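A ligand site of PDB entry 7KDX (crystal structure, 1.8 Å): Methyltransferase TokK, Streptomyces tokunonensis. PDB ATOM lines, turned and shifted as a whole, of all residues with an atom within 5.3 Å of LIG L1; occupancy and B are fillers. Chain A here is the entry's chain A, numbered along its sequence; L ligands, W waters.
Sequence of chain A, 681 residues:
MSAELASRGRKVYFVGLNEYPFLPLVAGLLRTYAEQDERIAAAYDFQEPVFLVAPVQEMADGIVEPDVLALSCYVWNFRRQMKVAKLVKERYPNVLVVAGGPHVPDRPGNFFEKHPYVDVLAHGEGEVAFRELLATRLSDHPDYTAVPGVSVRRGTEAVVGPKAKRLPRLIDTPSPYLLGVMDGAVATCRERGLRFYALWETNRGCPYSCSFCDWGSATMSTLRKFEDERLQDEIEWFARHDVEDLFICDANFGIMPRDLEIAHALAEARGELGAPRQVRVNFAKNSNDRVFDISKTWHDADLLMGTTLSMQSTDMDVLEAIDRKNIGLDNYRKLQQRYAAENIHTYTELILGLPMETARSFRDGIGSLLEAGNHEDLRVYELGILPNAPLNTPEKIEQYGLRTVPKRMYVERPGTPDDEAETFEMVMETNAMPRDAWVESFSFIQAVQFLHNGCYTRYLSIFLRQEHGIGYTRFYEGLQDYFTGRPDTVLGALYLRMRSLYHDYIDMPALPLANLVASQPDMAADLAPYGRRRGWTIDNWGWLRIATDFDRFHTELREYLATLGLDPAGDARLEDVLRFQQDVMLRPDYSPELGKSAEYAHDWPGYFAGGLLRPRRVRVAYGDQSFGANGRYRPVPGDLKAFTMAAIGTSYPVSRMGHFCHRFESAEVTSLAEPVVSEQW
N of Trp 215 is in hydrogen-bond range of O1 of LG2 L2. N of Gly 384 sits at hydrogen-bond distance from N1 of LIG L1 (3.2 Å). The backbone carbonyl oxygen (O) of Phe 212 is in hydrogen-bond range of a nitrogen (N5) of LIG L1, 3.1 Å away. OE1 of Glu 349 is in hydrogen-bond range of O3 of LIG L1 (2.8 Å). The side-chain amide oxygen of Gln 312 sits at hydrogen-bond distance from an oxygen (O2) of LIG L1 (2.7 Å). SG of Cys 213 binds FE4 of LG4 L4 (2.2 Å). The backbone carbonyl oxygen (O) of Gly 384 sits at hydrogen-bond distance from a nitrogen (N5) of LIG L1.
N4 of LIG L1 lies within hydrogen-bond range of N5 of LG2 L2 (3.1 Å). A sulfur (S1) of LG3 L3 lies close to an oxygen (O3) of LIG L1 (3.5 Å). A nitrogen (N1) of LG3 L3 is bound to an iron atom (FE3) of LG4 L4 (2.3 Å).
The backbone NH (N) of Tyr 381 lies within hydrogen-bond range of the backbone carbonyl oxygen (O) of Leu 350 (3.0 Å). OE2 of Glu 349 is in hydrogen-bond range of OH of Tyr 381 (2.6 Å). The backbone NH (N) of Ile 351 sits at hydrogen-bond distance from the backbone carbonyl oxygen (O) of Gln 312. The backbone NH (N) of Gln 312 is in hydrogen-bond range of the backbone carbonyl oxygen (O) of Glu 349, at 2.9 Å. The backbone NH (N) of Trp 215 lies close to the side-chain sulfur (SG) of Cys 213, at 3.5 Å. OG of Ser 310 is in hydrogen-bond range of OE1 of Glu 349 (2.6 Å).
CZ3 of Trp 215 touches C10 of LIG L1, at 3.6 Å. OD1 of Asn 282 touches C10 of LIG L1, 3.5 Å away. Ile 351 touches LIG L1 (CD1 to N2, 3.6 Å). Tyr 381 touches LIG L1. O of Glu 382 touches C1 of LIG L1, 3.2 Å away. Leu 383 touches LIG L1 (CD1 to N1, 3.9 Å). Leu 386 touches LIG L1. Hydrophobic or aromatic side chains that line LIG L1: Phe 212, Trp 215, Ile 351, Tyr 381, Leu 383 and Leu 386. Of the 15 residues printed, 11 come within 4 Å of LIG L1.
Water W1 lies within hydrogen-bond range of a nitrogen (N7) of LG2 L2 (2.6 Å) and an oxygen (O1) of LIG L1 (2.9 Å).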
ATOM      1  N   PHE A 212     -12.561   5.517   7.755  1.00  0.00           N
ATOM      2  CA  PHE A 212     -12.817   6.025   6.407  1.00  0.00           C
ATOM      3  C   PHE A 212     -13.810   7.185   6.381  1.00  0.00           C
ATOM      4  O   PHE A 212     -13.950   7.842   5.343  1.00  0.00           O
ATOM      5  CB  PHE A 212     -13.354   4.904   5.514  1.00  0.00           C
ATOM      6  CG  PHE A 212     -14.596   4.243   6.052  1.00  0.00           C
ATOM      7  CD1 PHE A 212     -15.842   4.827   5.870  1.00  0.00           C
ATOM      8  CD2 PHE A 212     -14.511   3.056   6.769  1.00  0.00           C
ATOM      9  CE1 PHE A 212     -16.976   4.240   6.386  1.00  0.00           C
ATOM     10  CE2 PHE A 212     -15.646   2.469   7.285  1.00  0.00           C
ATOM     11  CZ  PHE A 212     -16.881   3.056   7.094  1.00  0.00           C
ATOM     12  N   CYS A 213     -14.518   7.436   7.479  1.00  0.00           N
ATOM     13  CA  CYS A 213     -15.722   8.259   7.506  1.00  0.00           C
ATOM     14  C   CYS A 213     -15.420   9.660   8.016  1.00  0.00           C
ATOM     15  O   CYS A 213     -14.499   9.883   8.804  1.00  0.00           O
ATOM     16  CB  CYS A 213     -16.778   7.587   8.397  1.00  0.00           C
ATOM     17  SG  CYS A 213     -18.442   8.261   8.316  1.00  0.00           S
ATOM     18  N   TRP A 215     -18.501  11.767   8.660  1.00  0.00           N
ATOM     19  CA  TRP A 215     -19.925  12.098   8.665  1.00  0.00           C
ATOM     20  C   TRP A 215     -20.191  13.408   9.388  1.00  0.00           C
ATOM     21  O   TRP A 215     -19.932  13.524  10.592  1.00  0.00           O
ATOM     22  CB  TRP A 215     -20.711  10.976   9.320  1.00  0.00           C
ATOM     23  CG  TRP A 215     -22.156  10.946   8.952  1.00  0.00           C
ATOM     24  CD1 TRP A 215     -23.199  11.471   9.646  1.00  0.00           C
ATOM     25  CD2 TRP A 215     -22.708  10.345   7.779  1.00  0.00           C
ATOM     26  NE1 TRP A 215     -24.377  11.236   8.978  1.00  0.00           N
ATOM     27  CE2 TRP A 215     -24.099  10.550   7.829  1.00  0.00           C
ATOM     28  CE3 TRP A 215     -22.171   9.663   6.686  1.00  0.00           C
ATOM     29  CZ2 TRP A 215     -24.958  10.087   6.834  1.00  0.00           C
ATOM     30  CZ3 TRP A 215     -23.012   9.215   5.694  1.00  0.00           C
ATOM     31  CH2 TRP A 215     -24.391   9.432   5.777  1.00  0.00           C
ATOM     32  N   ASN A 282     -29.960   7.147   7.291  1.00  0.00           N
ATOM     33  CA  ASN A 282     -29.067   6.077   7.696  1.00  0.00           C
ATOM     34  C   ASN A 282     -29.440   5.630   9.105  1.00  0.00           C
ATOM     35  O   ASN A 282     -29.490   6.450  10.031  1.00  0.00           O
ATOM     36  CB  ASN A 282     -27.619   6.561   7.652  1.00  0.00           C
ATOM     37  CG  ASN A 282     -27.105   6.640   6.230  1.00  0.00           C
ATOM     38  OD1 ASN A 282     -26.590   5.659   5.706  1.00  0.00           O
ATOM     39  ND2 ASN A 282     -27.251   7.814   5.606  1.00  0.00           N
ATOM     40  N   SER A 310     -25.504  -1.974   7.907  1.00  0.00           N
ATOM     41  CA  SER A 310     -24.269  -1.967   7.136  1.00  0.00           C
ATOM     42  C   SER A 310     -23.099  -2.508   7.949  1.00  0.00           C
ATOM     43  O   SER A 310     -23.120  -2.539   9.187  1.00  0.00           O
ATOM     44  CB  SER A 310     -23.984  -0.550   6.645  1.00  0.00           C
ATOM     45  OG  SER A 310     -24.851  -0.247   5.573  1.00  0.00           O
ATOM     46  N   GLN A 312     -19.487  -2.569   6.150  1.00  0.00           N
ATOM     47  CA  GLN A 312     -18.251  -2.100   5.536  1.00  0.00           C
ATOM     48  C   GLN A 312     -17.321  -3.273   5.258  1.00  0.00           C
ATOM     49  O   GLN A 312     -16.822  -3.422   4.130  1.00  0.00           O
ATOM     50  CB  GLN A 312     -17.561  -1.027   6.401  1.00  0.00           C
ATOM     51  CG  GLN A 312     -18.501  -0.083   7.175  1.00  0.00           C
ATOM     52  CD  GLN A 312     -19.500   0.653   6.304  1.00  0.00           C
ATOM     53  OE1 GLN A 312     -19.463   0.583   5.079  1.00  0.00           O
ATOM     54  NE2 GLN A 312     -20.408   1.382   6.947  1.00  0.00           N
ATOM     55  N   GLU A 349     -24.240  -2.311   3.386  1.00  0.00           N
ATOM     56  CA  GLU A 349     -23.182  -1.684   2.606  1.00  0.00           C
ATOM     57  C   GLU A 349     -21.824  -2.284   2.943  1.00  0.00           C
ATOM     58  O   GLU A 349     -21.542  -2.592   4.103  1.00  0.00           O
ATOM     59  CB  GLU A 349     -23.145  -0.174   2.835  1.00  0.00           C
ATOM     60  CG  GLU A 349     -24.330   0.563   2.257  1.00  0.00           C
ATOM     61  CD  GLU A 349     -24.583   1.879   2.941  1.00  0.00           C
ATOM     62  OE1 GLU A 349     -24.468   1.945   4.179  1.00  0.00           O
ATOM     63  OE2 GLU A 349     -24.900   2.858   2.224  1.00  0.00           O
ATOM     64  N   LEU A 350     -20.996  -2.446   1.913  1.00  0.00           N
ATOM     65  CA  LEU A 350     -19.609  -2.844   2.033  1.00  0.00           C
ATOM     66  C   LEU A 350     -18.744  -1.836   1.288  1.00  0.00           C
ATOM     67  O   LEU A 350     -19.207  -1.180   0.349  1.00  0.00           O
ATOM     68  CB  LEU A 350     -19.367  -4.253   1.470  1.00  0.00           C
ATOM     69  CG  LEU A 350     -20.146  -5.423   2.091  1.00  0.00           C
ATOM     70  CD1 LEU A 350     -20.011  -6.675   1.242  1.00  0.00           C
ATOM     71  CD2 LEU A 350     -19.684  -5.690   3.514  1.00  0.00           C
ATOM     72  N   ILE A 351     -17.490  -1.707   1.705  1.00  0.00           N
ATOM     73  CA  ILE A 351     -16.519  -0.864   1.024  1.00  0.00           C
ATOM     74  C   ILE A 351     -15.375  -1.748   0.550  1.00  0.00           C
ATOM     75  O   ILE A 351     -14.837  -2.533   1.330  1.00  0.00           O
ATOM     76  CB  ILE A 351     -15.994   0.267   1.930  1.00  0.00           C
ATOM     77  CG1 ILE A 351     -17.146   1.190   2.353  1.00  0.00           C
ATOM     78  CG2 ILE A 351     -14.951   1.086   1.177  1.00  0.00           C
ATOM     79  CD1 ILE A 351     -16.734   2.205   3.384  1.00  0.00           C
ATOM     80  N   TYR A 381     -19.182   0.170  -2.310  1.00  0.00           N
ATOM     81  CA  TYR A 381     -18.592   1.429  -2.721  1.00  0.00           C
ATOM     82  C   TYR A 381     -17.089   1.284  -2.841  1.00  0.00           C
ATOM     83  O   TYR A 381     -16.459   0.594  -2.036  1.00  0.00           O
ATOM     84  CB  TYR A 381     -18.909   2.562  -1.727  1.00  0.00           C
ATOM     85  CG  TYR A 381     -20.367   2.680  -1.366  1.00  0.00           C
ATOM     86  CD1 TYR A 381     -21.315   3.025  -2.312  1.00  0.00           C
ATOM     87  CD2 TYR A 381     -20.785   2.472  -0.053  1.00  0.00           C
ATOM     88  CE1 TYR A 381     -22.653   3.137  -1.978  1.00  0.00           C
ATOM     89  CE2 TYR A 381     -22.117   2.583   0.287  1.00  0.00           C
ATOM     90  CZ  TYR A 381     -23.047   2.916  -0.665  1.00  0.00           C
ATOM     91  OH  TYR A 381     -24.372   3.024  -0.317  1.00  0.00           O
ATOM     92  N   GLU A 382     -16.511   1.932  -3.856  1.00  0.00           N
ATOM     93  CA  GLU A 382     -15.073   2.155  -3.882  1.00  0.00           C
ATOM     94  C   GLU A 382     -14.684   3.029  -2.704  1.00  0.00           C
ATOM     95  O   GLU A 382     -15.401   3.966  -2.355  1.00  0.00           O
ATOM     96  CB  GLU A 382     -14.644   2.858  -5.174  1.00  0.00           C
ATOM     97  CG  GLU A 382     -15.167   2.283  -6.463  1.00  0.00           C
ATOM     98  CD  GLU A 382     -16.442   2.929  -6.945  1.00  0.00           C
ATOM     99  OE1 GLU A 382     -17.382   3.115  -6.137  1.00  0.00           O
ATOM    100  OE2 GLU A 382     -16.513   3.261  -8.137  1.00  0.00           O
ATOM    101  N   LEU A 383     -13.530   2.740  -2.108  1.00  0.00           N
ATOM    102  CA  LEU A 383     -13.063   3.532  -0.983  1.00  0.00           C
ATOM    103  C   LEU A 383     -12.516   4.864  -1.487  1.00  0.00           C
ATOM    104  O   LEU A 383     -11.581   4.885  -2.286  1.00  0.00           O
ATOM    105  CB  LEU A 383     -12.009   2.768  -0.196  1.00  0.00           C
ATOM    106  CG  LEU A 383     -11.296   3.533   0.919  1.00  0.00           C
ATOM    107  CD1 LEU A 383     -12.284   4.113   1.923  1.00  0.00           C
ATOM    108  CD2 LEU A 383     -10.307   2.619   1.611  1.00  0.00           C
ATOM    109  N   GLY A 384     -13.092   5.962  -1.013  1.00  0.00           N
ATOM    110  CA  GLY A 384     -12.574   7.294  -1.297  1.00  0.00           C
ATOM    111  C   GLY A 384     -11.863   7.850  -0.074  1.00  0.00           C
ATOM    112  O   GLY A 384     -12.295   7.643   1.059  1.00  0.00           O
ATOM    113  N   ILE A 385     -10.751   8.553  -0.315  1.00  0.00           N
ATOM    114  CA  ILE A 385     -10.009   9.208   0.755  1.00  0.00           C
ATOM    115  C   ILE A 385     -10.613  10.588   0.963  1.00  0.00           C
ATOM    116  O   ILE A 385     -10.485  11.463   0.103  1.00  0.00           O
ATOM    117  CB  ILE A 385      -8.513   9.289   0.430  1.00  0.00           C
ATOM    118  CG1 ILE A 385      -7.921   7.898   0.203  1.00  0.00           C
ATOM    119  CG2 ILE A 385      -7.783  10.012   1.560  1.00  0.00           C
ATOM    120  CD1 ILE A 385      -7.989   6.994   1.428  1.00  0.00           C
ATOM    121  N   LEU A 386     -11.290  10.783   2.100  1.00  0.00           N
ATOM    122  CA  LEU A 386     -11.894  12.084   2.368  1.00  0.00           C
ATOM    123  C   LEU A 386     -10.892  12.977   3.092  1.00  0.00           C
ATOM    124  O   LEU A 386     -10.132  12.505   3.938  1.00  0.00           O
ATOM    125  CB  LEU A 386     -13.149  11.920   3.224  1.00  0.00           C
ATOM    126  CG  LEU A 386     -14.156  10.908   2.677  1.00  0.00           C
ATOM    127  CD1 LEU A 386     -15.374  10.772   3.589  1.00  0.00           C
ATOM    128  CD2 LEU A 386     -14.581  11.298   1.270  1.00  0.00           C
HETATM  129  N1  LIG L   1     -15.610   5.767   0.882  1.00  0.00           N
HETATM  130  C1  LIG L   1     -16.587   4.938   0.483  1.00  0.00           C
HETATM  131  N2  LIG L   1     -17.770   4.701   1.060  1.00  0.00           N
HETATM  132  C2  LIG L   1     -17.932   5.429   2.171  1.00  0.00           C
HETATM  133  N3  LIG L   1     -19.020   5.457   2.999  1.00  0.00           N
HETATM  134  C3  LIG L   1     -18.720   6.370   3.978  1.00  0.00           C
HETATM  135  N4  LIG L   1     -17.539   6.918   3.851  1.00  0.00           N
HETATM  136  C4  LIG L   1     -17.021   6.328   2.704  1.00  0.00           C
HETATM  137  C5  LIG L   1     -15.804   6.484   2.019  1.00  0.00           C
HETATM  138  N5  LIG L   1     -14.834   7.292   2.458  1.00  0.00           N
HETATM  139  C6  LIG L   1     -20.232   4.657   2.891  1.00  0.00           C
HETATM  140  C7  LIG L   1     -20.371   3.584   3.981  1.00  0.00           C
HETATM  141  C8  LIG L   1     -21.519   4.128   4.843  1.00  0.00           C
HETATM  142  C9  LIG L   1     -22.351   4.855   3.804  1.00  0.00           C
HETATM  143  C10 LIG L   1     -23.321   5.881   4.353  1.00  0.00           C
HETATM  144  O1  LIG L   1     -21.363   5.513   2.986  1.00  0.00           O
HETATM  145  O2  LIG L   1     -20.677   2.338   3.367  1.00  0.00           O
HETATM  146  O3  LIG L   1     -22.282   3.115   5.468  1.00  0.00           O
HETATM  147 CO1  LG2 L   2     -22.946  12.304   0.844  1.00  0.00          CO
HETATM  148  N1  LG2 L   2     -21.336  12.607   1.761  1.00  0.00           N
HETATM  149  N2  LG2 L   2     -21.983  11.397  -0.547  1.00  0.00           N
HETATM  150  N3  LG2 L   2     -24.584  12.550  -0.111  1.00  0.00           N
HETATM  151  N4  LG2 L   2     -23.740  13.022   2.401  1.00  0.00           N
HETATM  152  C1  LG2 L   2     -21.466  13.403   2.986  1.00  0.00           C
HETATM  153  C2  LG2 L   2     -21.552  14.882   2.643  1.00  0.00           C
HETATM  154  C3  LG2 L   2     -20.148  13.007   3.776  1.00  0.00           C
HETATM  155  C4  LG2 L   2     -19.670  14.051   4.797  1.00  0.00           C
HETATM  156  C5  LG2 L   2     -20.373  11.612   4.453  1.00  0.00           C
HETATM  157  C6  LG2 L   2     -19.093  10.815   4.763  1.00  0.00           C
HETATM  158  O1  LG2 L   2     -18.260  11.298   5.538  1.00  0.00           O
HETATM  159  N5  LG2 L   2     -18.946   9.625   4.197  1.00  0.00           N
HETATM  160  C7  LG2 L   2     -19.169  12.763   2.573  1.00  0.00           C
HETATM  161  C8  LG2 L   2     -18.502  14.009   1.950  1.00  0.00           C
HETATM  162  C9  LG2 L   2     -17.060  14.270   2.386  1.00  0.00           C
HETATM  163  C10 LG2 L   2     -16.432  15.352   1.531  1.00  0.00           C
HETATM  164  O2  LG2 L   2     -17.033  15.835   0.572  1.00  0.00           O
HETATM  165  N6  LG2 L   2     -15.211  15.746   1.889  1.00  0.00           N
HETATM  166  C11 LG2 L   2     -20.113  12.230   1.525  1.00  0.00           C
HETATM  167  C12 LG2 L   2     -19.753  11.387   0.368  1.00  0.00           C
HETATM  168  C13 LG2 L   2     -18.300  10.984   0.427  1.00  0.00           C
HETATM  169  C14 LG2 L   2     -20.640  11.101  -0.647  1.00  0.00           C
HETATM  170  C15 LG2 L   2     -20.363  10.438  -1.996  1.00  0.00           C
HETATM  171  C16 LG2 L   2     -19.565  11.431  -2.864  1.00  0.00           C
HETATM  172  C17 LG2 L   2     -19.596   9.095  -1.802  1.00  0.00           C
HETATM  173  C18 LG2 L   2     -20.159   8.025  -0.838  1.00  0.00           C
HETATM  174  O3  LG2 L   2     -19.578   6.928  -0.807  1.00  0.00           O
HETATM  175  N7  LG2 L   2     -21.215   8.288  -0.083  1.00  0.00           N
HETATM  176  C19 LG2 L   2     -21.772  10.133  -2.584  1.00  0.00           C
HETATM  177  C20 LG2 L   2     -21.963  10.426  -4.080  1.00  0.00           C
HETATM  178  C21 LG2 L   2     -21.415   9.322  -4.985  1.00  0.00           C
HETATM  179  C22 LG2 L   2     -21.809   9.460  -6.436  1.00  0.00           C
HETATM  180  O4  LG2 L   2     -22.106  10.555  -6.918  1.00  0.00           O
HETATM  181  N8  LG2 L   2     -21.826   8.340  -7.152  1.00  0.00           N
HETATM  182  C23 LG2 L   2     -22.640  10.975  -1.671  1.00  0.00           C
HETATM  183  C24 LG2 L   2     -23.964  11.205  -1.991  1.00  0.00           C
HETATM  184  C25 LG2 L   2     -24.884  11.937  -1.269  1.00  0.00           C
HETATM  185  C26 LG2 L   2     -26.328  12.134  -1.669  1.00  0.00           C
HETATM  186  C27 LG2 L   2     -27.239  11.025  -1.117  1.00  0.00           C
HETATM  187  C28 LG2 L   2     -26.515  12.228  -3.196  1.00  0.00           C
HETATM  188  C29 LG2 L   2     -26.630  13.443  -0.886  1.00  0.00           C
HETATM  189  C30 LG2 L   2     -26.220  14.744  -1.606  1.00  0.00           C
HETATM  190  C31 LG2 L   2     -26.470  16.004  -0.802  1.00  0.00           C
HETATM  191  C32 LG2 L   2     -26.243  17.275  -1.598  1.00  0.00           C
HETATM  192  O5  LG2 L   2     -26.119  18.368  -1.028  1.00  0.00           O
HETATM  193  N9  LG2 L   2     -26.190  17.139  -2.912  1.00  0.00           N
HETATM  194  C33 LG2 L   2     -25.721  13.274   0.351  1.00  0.00           C
HETATM  195  C34 LG2 L   2     -25.918  13.657   1.659  1.00  0.00           C
HETATM  196  C35 LG2 L   2     -27.260  14.250   1.966  1.00  0.00           C
HETATM  197  C36 LG2 L   2     -24.914  13.508   2.720  1.00  0.00           C
HETATM  198  C37 LG2 L   2     -24.998  13.822   4.208  1.00  0.00           C
HETATM  199  C38 LG2 L   2     -25.763  12.667   4.876  1.00  0.00           C
HETATM  200  C39 LG2 L   2     -25.673  15.166   4.580  1.00  0.00           C
HETATM  201  C40 LG2 L   2     -25.049  16.462   4.065  1.00  0.00           C
HETATM  202  C41 LG2 L   2     -25.720  17.666   4.697  1.00  0.00           C
HETATM  203  O6  LG2 L   2     -26.473  18.384   4.053  1.00  0.00           O
HETATM  204  N10 LG2 L   2     -25.477  17.849   5.990  1.00  0.00           N
HETATM  205  C42 LG2 L   2     -23.496  13.868   4.584  1.00  0.00           C
HETATM  206  C43 LG2 L   2     -23.179  13.509   6.056  1.00  0.00           C
HETATM  207  C44 LG2 L   2     -23.612  14.604   7.007  1.00  0.00           C
HETATM  208  O7  LG2 L   2     -23.169  15.748   6.889  1.00  0.00           O
HETATM  209  N11 LG2 L   2     -24.485  14.260   7.935  1.00  0.00           N
HETATM  210  C45 LG2 L   2     -22.824  12.957   3.552  1.00  0.00           C
HETATM  211  C46 LG2 L   2     -26.126  18.878   6.787  1.00  0.00           C
HETATM  212  C47 LG2 L   2     -25.305  20.131   6.854  1.00  0.00           C
HETATM  213  C48 LG2 L   2     -26.085  21.197   7.586  1.00  0.00           C
HETATM  214  O8  LG2 L   2     -24.164  19.850   7.602  1.00  0.00           O
HETATM  215  O9  LG2 L   2     -22.498  19.472   5.683  1.00  0.00           O
HETATM  216  O10 LG2 L   2     -21.743  19.417   8.100  1.00  0.00           O
HETATM  217  P1  LG2 L   2     -22.676  20.023   7.048  1.00  0.00           P
HETATM  218  O11 LG2 L   2     -22.529  21.635   7.083  1.00  0.00           O
HETATM  219  C49 LG2 L   2     -21.949  22.308   8.182  1.00  0.00           C
HETATM  220  C50 LG2 L   2     -20.424  22.496   8.122  1.00  0.00           C
HETATM  221  O12 LG2 L   2     -19.846  21.719   7.075  1.00  0.00           O
HETATM  222  C51 LG2 L   2     -20.284  24.012   7.888  1.00  0.00           C
HETATM  223  O13 LG2 L   2     -21.409  24.598   8.494  1.00  0.00           O
HETATM  224  C52 LG2 L   2     -22.529  23.723   8.295  1.00  0.00           C
HETATM  225  C53 LG2 L   2     -23.534  23.923   9.400  1.00  0.00           C
HETATM  226  O14 LG2 L   2     -22.948  23.691  10.677  1.00  0.00           O
HETATM  227  N12 LG2 L   2     -20.206  24.444   6.492  1.00  0.00           N
HETATM  228  C54 LG2 L   2     -19.823  25.731   6.138  1.00  0.00           C
HETATM  229  C55 LG2 L   2     -20.698  23.867   5.368  1.00  0.00           C
HETATM  230  N13 LG2 L   2     -20.670  24.646   4.309  1.00  0.00           N
HETATM  231  C56 LG2 L   2     -20.114  25.830   4.776  1.00  0.00           C
HETATM  232  C57 LG2 L   2     -19.853  27.032   4.122  1.00  0.00           C
HETATM  233  C58 LG2 L   2     -19.340  28.120   4.821  1.00  0.00           C
HETATM  234  C59 LG2 L   2     -19.075  29.405   4.077  1.00  0.00           C
HETATM  235  C60 LG2 L   2     -19.081  28.010   6.209  1.00  0.00           C
HETATM  236  C61 LG2 L   2     -18.593  29.193   6.999  1.00  0.00           C
HETATM  237  C62 LG2 L   2     -19.320  26.805   6.855  1.00  0.00           C
HETATM  238  N1  LG3 L   3     -23.758   4.750  11.087  1.00  0.00           N
HETATM  239  C1  LG3 L   3     -24.414   3.591  10.483  1.00  0.00           C
HETATM  240  C2  LG3 L   3     -23.381   2.526  10.169  1.00  0.00           C
HETATM  241  O1  LG3 L   3     -22.197   2.844   9.974  1.00  0.00           O
HETATM  242  C3  LG3 L   3     -25.165   3.978   9.206  1.00  0.00           C
HETATM  243  C4  LG3 L   3     -24.283   4.064   7.962  1.00  0.00           C
HETATM  244  S1  LG3 L   3     -23.009   5.354   8.002  1.00  0.00           S
HETATM  245  C5  LG3 L   3     -24.036   6.818   8.175  1.00  0.00           C
HETATM  246  O2  LG3 L   3     -23.688   1.332  10.109  1.00  0.00           O
HETATM  247 FE1  LG4 L   4     -18.983   4.648  11.227  1.00  0.00          FE
HETATM  248 FE2  LG4 L   4     -20.400   6.691  12.318  1.00  0.00          FE
HETATM  249 FE3  LG4 L   4     -21.578   5.090  10.297  1.00  0.00          FE
HETATM  250 FE4  LG4 L   4     -19.505   6.884   9.743  1.00  0.00          FE
HETATM  251  S1  LG4 L   4     -21.577   7.420  10.461  1.00  0.00           S
HETATM  252  S2  LG4 L   4     -19.702   4.699   9.026  1.00  0.00           S
HETATM  253  S3  LG4 L   4     -18.243   6.758  11.666  1.00  0.00           S
HETATM  254  S4  LG4 L   4     -20.874   4.447  12.455  1.00  0.00           S
HETATM  255  O   HOH W   1     -20.966   8.338   2.531  1.00  0.00           O
